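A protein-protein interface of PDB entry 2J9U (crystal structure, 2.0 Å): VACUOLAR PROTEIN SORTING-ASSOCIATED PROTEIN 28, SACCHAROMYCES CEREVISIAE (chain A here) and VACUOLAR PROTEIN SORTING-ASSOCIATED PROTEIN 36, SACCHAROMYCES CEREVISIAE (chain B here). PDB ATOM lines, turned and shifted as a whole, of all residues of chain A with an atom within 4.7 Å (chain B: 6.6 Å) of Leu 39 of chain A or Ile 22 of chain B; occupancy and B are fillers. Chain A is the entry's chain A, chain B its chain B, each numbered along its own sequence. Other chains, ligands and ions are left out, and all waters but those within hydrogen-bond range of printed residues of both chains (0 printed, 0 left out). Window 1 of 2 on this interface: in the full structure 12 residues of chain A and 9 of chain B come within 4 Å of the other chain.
Printed residues of chain B within 4 Å of Ile 40 of chain A: Ile 22 (3.8 Å), Val 48 (3.7 Å) and Leu 54 (3.9 Å).
Printed residues of chain B within 4 Å of Asn 43 of chain A: Pro 21 and Leu 54.
Printed residues of chain B within 4 Å of Ile 60 of chain A: Val 48.
Cys 20 of chain B touches none of the printed residues of chain A.
Printed residues of chain A within 4 Å of Pro 21 of chain B: Asn 43 (3.9 Å).
Of chain A, only Leu 39, Ile 40 and Ile 57 come within 4 Å of Ile 22 of chain B.
Met 24 of chain B touches none of the printed residues of chain A.
Printed residues of chain A within 4 Å of Leu 54 of chain B: Ile 40 (3.9 Å) and Asn 43 (3.8 Å).
The nearest residue of chain B that does not touch Leu 39 of chain A is Leu 54 of chain B (5.6 Å).
Printed residues of chain B that touch a printed residue of chain A: Pro 21, Ile 22, Cys 23, Val 48 and Leu 54.
Hydrophobic or aromatic side chains of chain B within 4 Å of the printed part of chain A: Ile 22, Val 48 and Leu 54.
Among the printed residues, 10 pairs touch across the chains.
Among the printed residues, no Asp or Glu carboxylate lies within 4 Å of a Lys or Arg side-chain nitrogen of the other chain.
The side-chain amide nitrogen (ND2) of Asn 43 of chain A sits at hydrogen-bond distance from the backbone carbonyl oxygen (O) of Leu 39 of chain A (3.0 Å).
The backbone NH of Ile 22 of chain B lies close to the side-chain sulfur of Cys 20 of chain B.
N of Val 48 of chain B lies close to SG of Cys 46 of chain B.
Among the printed residues, merely in contact across the chains: Ala 36 of chain A with Val 48 of chain B, Leu 39 of chain A with Ile 22 of chain B, Ile 40 of chain A with Ile 22 of chain B, Ile 40 of chain A with Val 48 of chain B, Ile 40 of chain A with Leu 54 of chain B, Asn 43 of chain A with Pro 21 of chain B, Asn 43 of chain A with Leu 54 of chain B, Ile 57 of chain A with Ile 22 of chain B, Ile 57 of chain A with Cys 23 of chain B and Ile 60 of chain A with Val 48 of chain B.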
ATOM      1  N   LEU A  35       6.521   4.027 -29.183  1.00  0.00           N
ATOM      2  CA  LEU A  35       7.661   4.729 -28.608  1.00  0.00           C
ATOM      3  C   LEU A  35       7.515   4.860 -27.117  1.00  0.00           C
ATOM      4  O   LEU A  35       8.509   4.732 -26.405  1.00  0.00           O
ATOM      5  CB  LEU A  35       7.891   6.112 -29.252  1.00  0.00           C
ATOM      6  CG  LEU A  35       8.446   6.148 -30.661  1.00  0.00           C
ATOM      7  CD1 LEU A  35       8.454   7.589 -31.222  1.00  0.00           C
ATOM      8  CD2 LEU A  35       9.859   5.546 -30.716  1.00  0.00           C
ATOM      9  N   ALA A  36       6.287   5.064 -26.625  1.00  0.00           N
ATOM     10  CA  ALA A  36       6.053   5.181 -25.154  1.00  0.00           C
ATOM     11  C   ALA A  36       6.497   3.876 -24.445  1.00  0.00           C
ATOM     12  O   ALA A  36       7.276   3.912 -23.478  1.00  0.00           O
ATOM     13  CB  ALA A  36       4.632   5.477 -24.848  1.00  0.00           C
ATOM     14  N   GLU A  37       5.994   2.731 -24.934  1.00  0.00           N
ATOM     15  CA  GLU A  37       6.337   1.473 -24.339  1.00  0.00           C
ATOM     16  C   GLU A  37       7.853   1.148 -24.472  1.00  0.00           C
ATOM     17  O   GLU A  37       8.459   0.609 -23.532  1.00  0.00           O
ATOM     18  CB  GLU A  37       5.465   0.339 -24.904  1.00  0.00           C
ATOM     19  CG  GLU A  37       5.491  -0.974 -24.067  1.00  0.00           C
ATOM     20  CD  GLU A  37       5.364  -0.787 -22.523  1.00  0.00           C
ATOM     21  OE1 GLU A  37       4.360  -0.200 -22.045  1.00  0.00           O
ATOM     22  OE2 GLU A  37       6.285  -1.237 -21.776  1.00  0.00           O
ATOM     23  N   LEU A  38       8.453   1.487 -25.613  1.00  0.00           N
ATOM     24  CA  LEU A  38       9.920   1.389 -25.750  1.00  0.00           C
ATOM     25  C   LEU A  38      10.670   2.149 -24.637  1.00  0.00           C
ATOM     26  O   LEU A  38      11.518   1.611 -23.921  1.00  0.00           O
ATOM     27  CB  LEU A  38      10.372   1.819 -27.182  1.00  0.00           C
ATOM     28  CG  LEU A  38      11.887   1.855 -27.355  1.00  0.00           C
ATOM     29  CD1 LEU A  38      12.579   0.412 -27.111  1.00  0.00           C
ATOM     30  CD2 LEU A  38      12.244   2.352 -28.795  1.00  0.00           C
ATOM     31  N   LEU A  39      10.336   3.422 -24.467  1.00  0.00           N
ATOM     32  CA  LEU A  39      11.072   4.270 -23.509  1.00  0.00           C
ATOM     33  C   LEU A  39      10.859   3.813 -22.046  1.00  0.00           C
ATOM     34  O   LEU A  39      11.777   3.847 -21.217  1.00  0.00           O
ATOM     35  CB  LEU A  39      10.660   5.735 -23.727  1.00  0.00           C
ATOM     36  CG  LEU A  39      11.226   6.295 -25.050  1.00  0.00           C
ATOM     37  CD1 LEU A  39      10.641   7.700 -25.324  1.00  0.00           C
ATOM     38  CD2 LEU A  39      12.760   6.300 -25.073  1.00  0.00           C
ATOM     39  N   ILE A  40       9.645   3.387 -21.730  1.00  0.00           N
ATOM     40  CA  ILE A  40       9.383   2.784 -20.422  1.00  0.00           C
ATOM     41  C   ILE A  40      10.268   1.517 -20.178  1.00  0.00           C
ATOM     42  O   ILE A  40      10.907   1.373 -19.068  1.00  0.00           O
ATOM     43  CB  ILE A  40       7.854   2.442 -20.206  1.00  0.00           C
ATOM     44  CG1 ILE A  40       7.000   3.719 -20.078  1.00  0.00           C
ATOM     45  CG2 ILE A  40       7.672   1.601 -18.897  1.00  0.00           C
ATOM     46  CD1 ILE A  40       5.478   3.506 -20.105  1.00  0.00           C
ATOM     47  N   SER A  41      10.310   0.604 -21.174  1.00  0.00           N
ATOM     48  CA  SER A  41      11.049  -0.673 -21.028  1.00  0.00           C
ATOM     49  C   SER A  41      12.553  -0.393 -20.903  1.00  0.00           C
ATOM     50  O   SER A  41      13.252  -1.033 -20.125  1.00  0.00           O
ATOM     51  CB  SER A  41      10.756  -1.623 -22.203  1.00  0.00           C
ATOM     52  OG  SER A  41      11.250  -1.090 -23.442  1.00  0.00           O
ATOM     53  N   ILE A  42      13.062   0.604 -21.643  1.00  0.00           N
ATOM     54  CA  ILE A  42      14.486   0.958 -21.570  1.00  0.00           C
ATOM     55  C   ILE A  42      14.870   1.406 -20.113  1.00  0.00           C
ATOM     56  O   ILE A  42      15.891   0.984 -19.518  1.00  0.00           O
ATOM     57  CB  ILE A  42      14.818   2.067 -22.583  1.00  0.00           C
ATOM     58  CG1 ILE A  42      14.875   1.508 -24.026  1.00  0.00           C
ATOM     59  CG2 ILE A  42      16.132   2.776 -22.266  1.00  0.00           C
ATOM     60  CD1 ILE A  42      14.934   2.653 -25.099  1.00  0.00           C
ATOM     61  N   ASN A  43      14.040   2.282 -19.541  1.00  0.00           N
ATOM     62  CA  ASN A  43      14.275   2.781 -18.175  1.00  0.00           C
ATOM     63  C   ASN A  43      14.203   1.693 -17.102  1.00  0.00           C
ATOM     64  O   ASN A  43      14.868   1.839 -16.083  1.00  0.00           O
ATOM     65  CB  ASN A  43      13.356   3.982 -17.845  1.00  0.00           C
ATOM     66  CG  ASN A  43      13.889   5.303 -18.400  1.00  0.00           C
ATOM     67  OD1 ASN A  43      14.805   5.906 -17.835  1.00  0.00           O
ATOM     68  ND2 ASN A  43      13.302   5.777 -19.512  1.00  0.00           N
ATOM     69  N   LEU A  56      15.626   9.927 -28.847  1.00  0.00           N
ATOM     70  CA  LEU A  56      14.361   9.214 -28.869  1.00  0.00           C
ATOM     71  C   LEU A  56      13.332   9.927 -27.983  1.00  0.00           C
ATOM     72  O   LEU A  56      12.119   9.982 -28.307  1.00  0.00           O
ATOM     73  CB  LEU A  56      14.535   7.767 -28.402  1.00  0.00           C
ATOM     74  CG  LEU A  56      15.442   6.852 -29.265  1.00  0.00           C
ATOM     75  CD1 LEU A  56      15.387   5.426 -28.755  1.00  0.00           C
ATOM     76  CD2 LEU A  56      15.117   6.942 -30.830  1.00  0.00           C
ATOM     77  N   ILE A  57      13.795  10.464 -26.859  1.00  0.00           N
ATOM     78  CA  ILE A  57      12.961  11.385 -26.050  1.00  0.00           C
ATOM     79  C   ILE A  57      12.422  12.594 -26.877  1.00  0.00           C
ATOM     80  O   ILE A  57      11.203  12.888 -26.847  1.00  0.00           O
ATOM     81  CB  ILE A  57      13.644  11.816 -24.729  1.00  0.00           C
ATOM     82  CG1 ILE A  57      13.955  10.563 -23.871  1.00  0.00           C
ATOM     83  CG2 ILE A  57      12.702  12.778 -23.911  1.00  0.00           C
ATOM     84  CD1 ILE A  57      15.039  10.735 -22.774  1.00  0.00           C
ATOM     85  N   ILE A  60       9.542  11.420 -29.222  1.00  0.00           N
ATOM     86  CA  ILE A  60       8.226  11.199 -28.654  1.00  0.00           C
ATOM     87  C   ILE A  60       7.532  12.542 -28.207  1.00  0.00           C
ATOM     88  O   ILE A  60       6.323  12.683 -28.381  1.00  0.00           O
ATOM     89  CB  ILE A  60       8.219  10.123 -27.558  1.00  0.00           C
ATOM     90  CG1 ILE A  60       6.753   9.632 -27.405  1.00  0.00           C
ATOM     91  CG2 ILE A  60       8.755  10.739 -26.257  1.00  0.00           C
ATOM     92  CD1 ILE A  60       6.509   8.572 -26.437  1.00  0.00           C
ATOM     93  N   VAL B  19       7.716  13.793 -11.051  1.00  0.00           N
ATOM     94  CA  VAL B  19       8.530  14.077 -12.239  1.00  0.00           C
ATOM     95  C   VAL B  19       8.491  12.927 -13.253  1.00  0.00           C
ATOM     96  O   VAL B  19       8.685  11.776 -12.893  1.00  0.00           O
ATOM     97  CB  VAL B  19       9.956  14.564 -11.867  1.00  0.00           C
ATOM     98  CG1 VAL B  19      10.361  14.043 -10.541  1.00  0.00           C
ATOM     99  CG2 VAL B  19      11.022  14.291 -12.929  1.00  0.00           C
ATOM    100  N   CYS B  20       8.200  13.262 -14.523  1.00  0.00           N
ATOM    101  CA  CYS B  20       8.083  12.251 -15.555  1.00  0.00           C
ATOM    102  C   CYS B  20       9.436  11.515 -15.692  1.00  0.00           C
ATOM    103  O   CYS B  20      10.465  12.151 -15.939  1.00  0.00           O
ATOM    104  CB  CYS B  20       7.688  12.889 -16.888  1.00  0.00           C
ATOM    105  SG  CYS B  20       7.627  11.697 -18.220  1.00  0.00           S
ATOM    106  N   PRO B  21       9.436  10.167 -15.547  1.00  0.00           N
ATOM    107  CA  PRO B  21      10.703   9.398 -15.683  1.00  0.00           C
ATOM    108  C   PRO B  21      11.179   9.312 -17.139  1.00  0.00           C
ATOM    109  O   PRO B  21      12.311   8.954 -17.398  1.00  0.00           O
ATOM    110  CB  PRO B  21      10.336   8.014 -15.150  1.00  0.00           C
ATOM    111  CG  PRO B  21       8.840   7.856 -15.413  1.00  0.00           C
ATOM    112  CD  PRO B  21       8.263   9.291 -15.290  1.00  0.00           C
ATOM    113  N   ILE B  22      10.312   9.675 -18.089  1.00  0.00           N
ATOM    114  CA  ILE B  22      10.708   9.646 -19.503  1.00  0.00           C
ATOM    115  C   ILE B  22      11.448  10.922 -19.901  1.00  0.00           C
ATOM    116  O   ILE B  22      12.569  10.833 -20.383  1.00  0.00           O
ATOM    117  CB  ILE B  22       9.491   9.409 -20.427  1.00  0.00           C
ATOM    118  CG1 ILE B  22       8.676   8.192 -19.946  1.00  0.00           C
ATOM    119  CG2 ILE B  22       9.912   9.294 -21.916  1.00  0.00           C
ATOM    120  CD1 ILE B  22       9.379   6.828 -20.077  1.00  0.00           C
ATOM    121  N   CYS B  23      10.801  12.089 -19.693  1.00  0.00           N
ATOM    122  CA  CYS B  23      11.297  13.381 -20.170  1.00  0.00           C
ATOM    123  C   CYS B  23      11.772  14.341 -19.066  1.00  0.00           C
ATOM    124  O   CYS B  23      12.392  15.364 -19.369  1.00  0.00           O
ATOM    125  CB  CYS B  23      10.255  14.066 -21.050  1.00  0.00           C
ATOM    126  SG  CYS B  23       8.785  14.720 -20.194  1.00  0.00           S
ATOM    127  N   MET B  24      11.483  14.006 -17.807  1.00  0.00           N
ATOM    128  CA  MET B  24      11.990  14.739 -16.645  1.00  0.00           C
ATOM    129  C   MET B  24      11.267  16.051 -16.314  1.00  0.00           C
ATOM    130  O   MET B  24      11.770  16.835 -15.502  1.00  0.00           O
ATOM    131  CB  MET B  24      13.491  15.017 -16.798  1.00  0.00           C
ATOM    132  CG  MET B  24      14.400  14.326 -15.822  1.00  0.00           C
ATOM    133  SD  MET B  24      14.478  12.546 -15.710  1.00  0.00           S
ATOM    134  CE  MET B  24      13.158  12.044 -14.637  1.00  0.00           C
ATOM    135  N   VAL B  25      10.113  16.300 -16.936  1.00  0.00           N
ATOM    136  CA  VAL B  25       9.344  17.497 -16.601  1.00  0.00           C
ATOM    137  C   VAL B  25       8.438  17.272 -15.389  1.00  0.00           C
ATOM    138  O   VAL B  25       7.915  16.188 -15.192  1.00  0.00           O
ATOM    139  CB  VAL B  25       8.585  18.219 -17.808  1.00  0.00           C
ATOM    140  CG1 VAL B  25       9.287  18.107 -19.169  1.00  0.00           C
ATOM    141  CG2 VAL B  25       7.086  17.981 -17.824  1.00  0.00           C
ATOM    142  N   CYS B  46       5.281  14.797 -22.830  1.00  0.00           N
ATOM    143  CA  CYS B  46       5.582  13.694 -23.781  1.00  0.00           C
ATOM    144  C   CYS B  46       4.362  12.799 -23.953  1.00  0.00           C
ATOM    145  O   CYS B  46       4.307  11.961 -24.861  1.00  0.00           O
ATOM    146  CB  CYS B  46       6.801  12.866 -23.288  1.00  0.00           C
ATOM    147  SG  CYS B  46       6.462  11.923 -21.754  1.00  0.00           S
ATOM    148  N   VAL B  48       3.278  10.328 -22.165  1.00  0.00           N
ATOM    149  CA  VAL B  48       3.399   8.934 -21.702  1.00  0.00           C
ATOM    150  C   VAL B  48       2.697   8.796 -20.341  1.00  0.00           C
ATOM    151  O   VAL B  48       2.948   9.605 -19.458  1.00  0.00           O
ATOM    152  CB  VAL B  48       4.897   8.528 -21.627  1.00  0.00           C
ATOM    153  CG1 VAL B  48       5.076   7.072 -21.094  1.00  0.00           C
ATOM    154  CG2 VAL B  48       5.548   8.707 -23.014  1.00  0.00           C
ATOM    155  N   PRO B  49       1.760   7.805 -20.184  1.00  0.00           N
ATOM    156  CA  PRO B  49       1.203   7.496 -18.849  1.00  0.00           C
ATOM    157  C   PRO B  49       2.313   7.158 -17.834  1.00  0.00           C
ATOM    158  O   PRO B  49       3.182   6.320 -18.119  1.00  0.00           O
ATOM    159  CB  PRO B  49       0.385   6.243 -19.094  1.00  0.00           C
ATOM    160  CG  PRO B  49       0.078   6.281 -20.578  1.00  0.00           C
ATOM    161  CD  PRO B  49       1.258   6.888 -21.223  1.00  0.00           C
ATOM    162  N   LEU B  54       8.646   3.407 -11.673  1.00  0.00           N
ATOM    163  CA  LEU B  54       9.684   4.378 -12.074  1.00  0.00           C
ATOM    164  C   LEU B  54       9.517   5.778 -11.474  1.00  0.00           C
ATOM    165  O   LEU B  54      10.490   6.511 -11.374  1.00  0.00           O
ATOM    166  CB  LEU B  54       9.772   4.500 -13.610  1.00  0.00           C
ATOM    167  CG  LEU B  54      10.285   3.280 -14.360  1.00  0.00           C
ATOM    168  CD1 LEU B  54      10.174   3.483 -15.875  1.00  0.00           C
ATOM    169  CD2 LEU B  54      11.750   3.032 -13.942  1.00  0.00           C
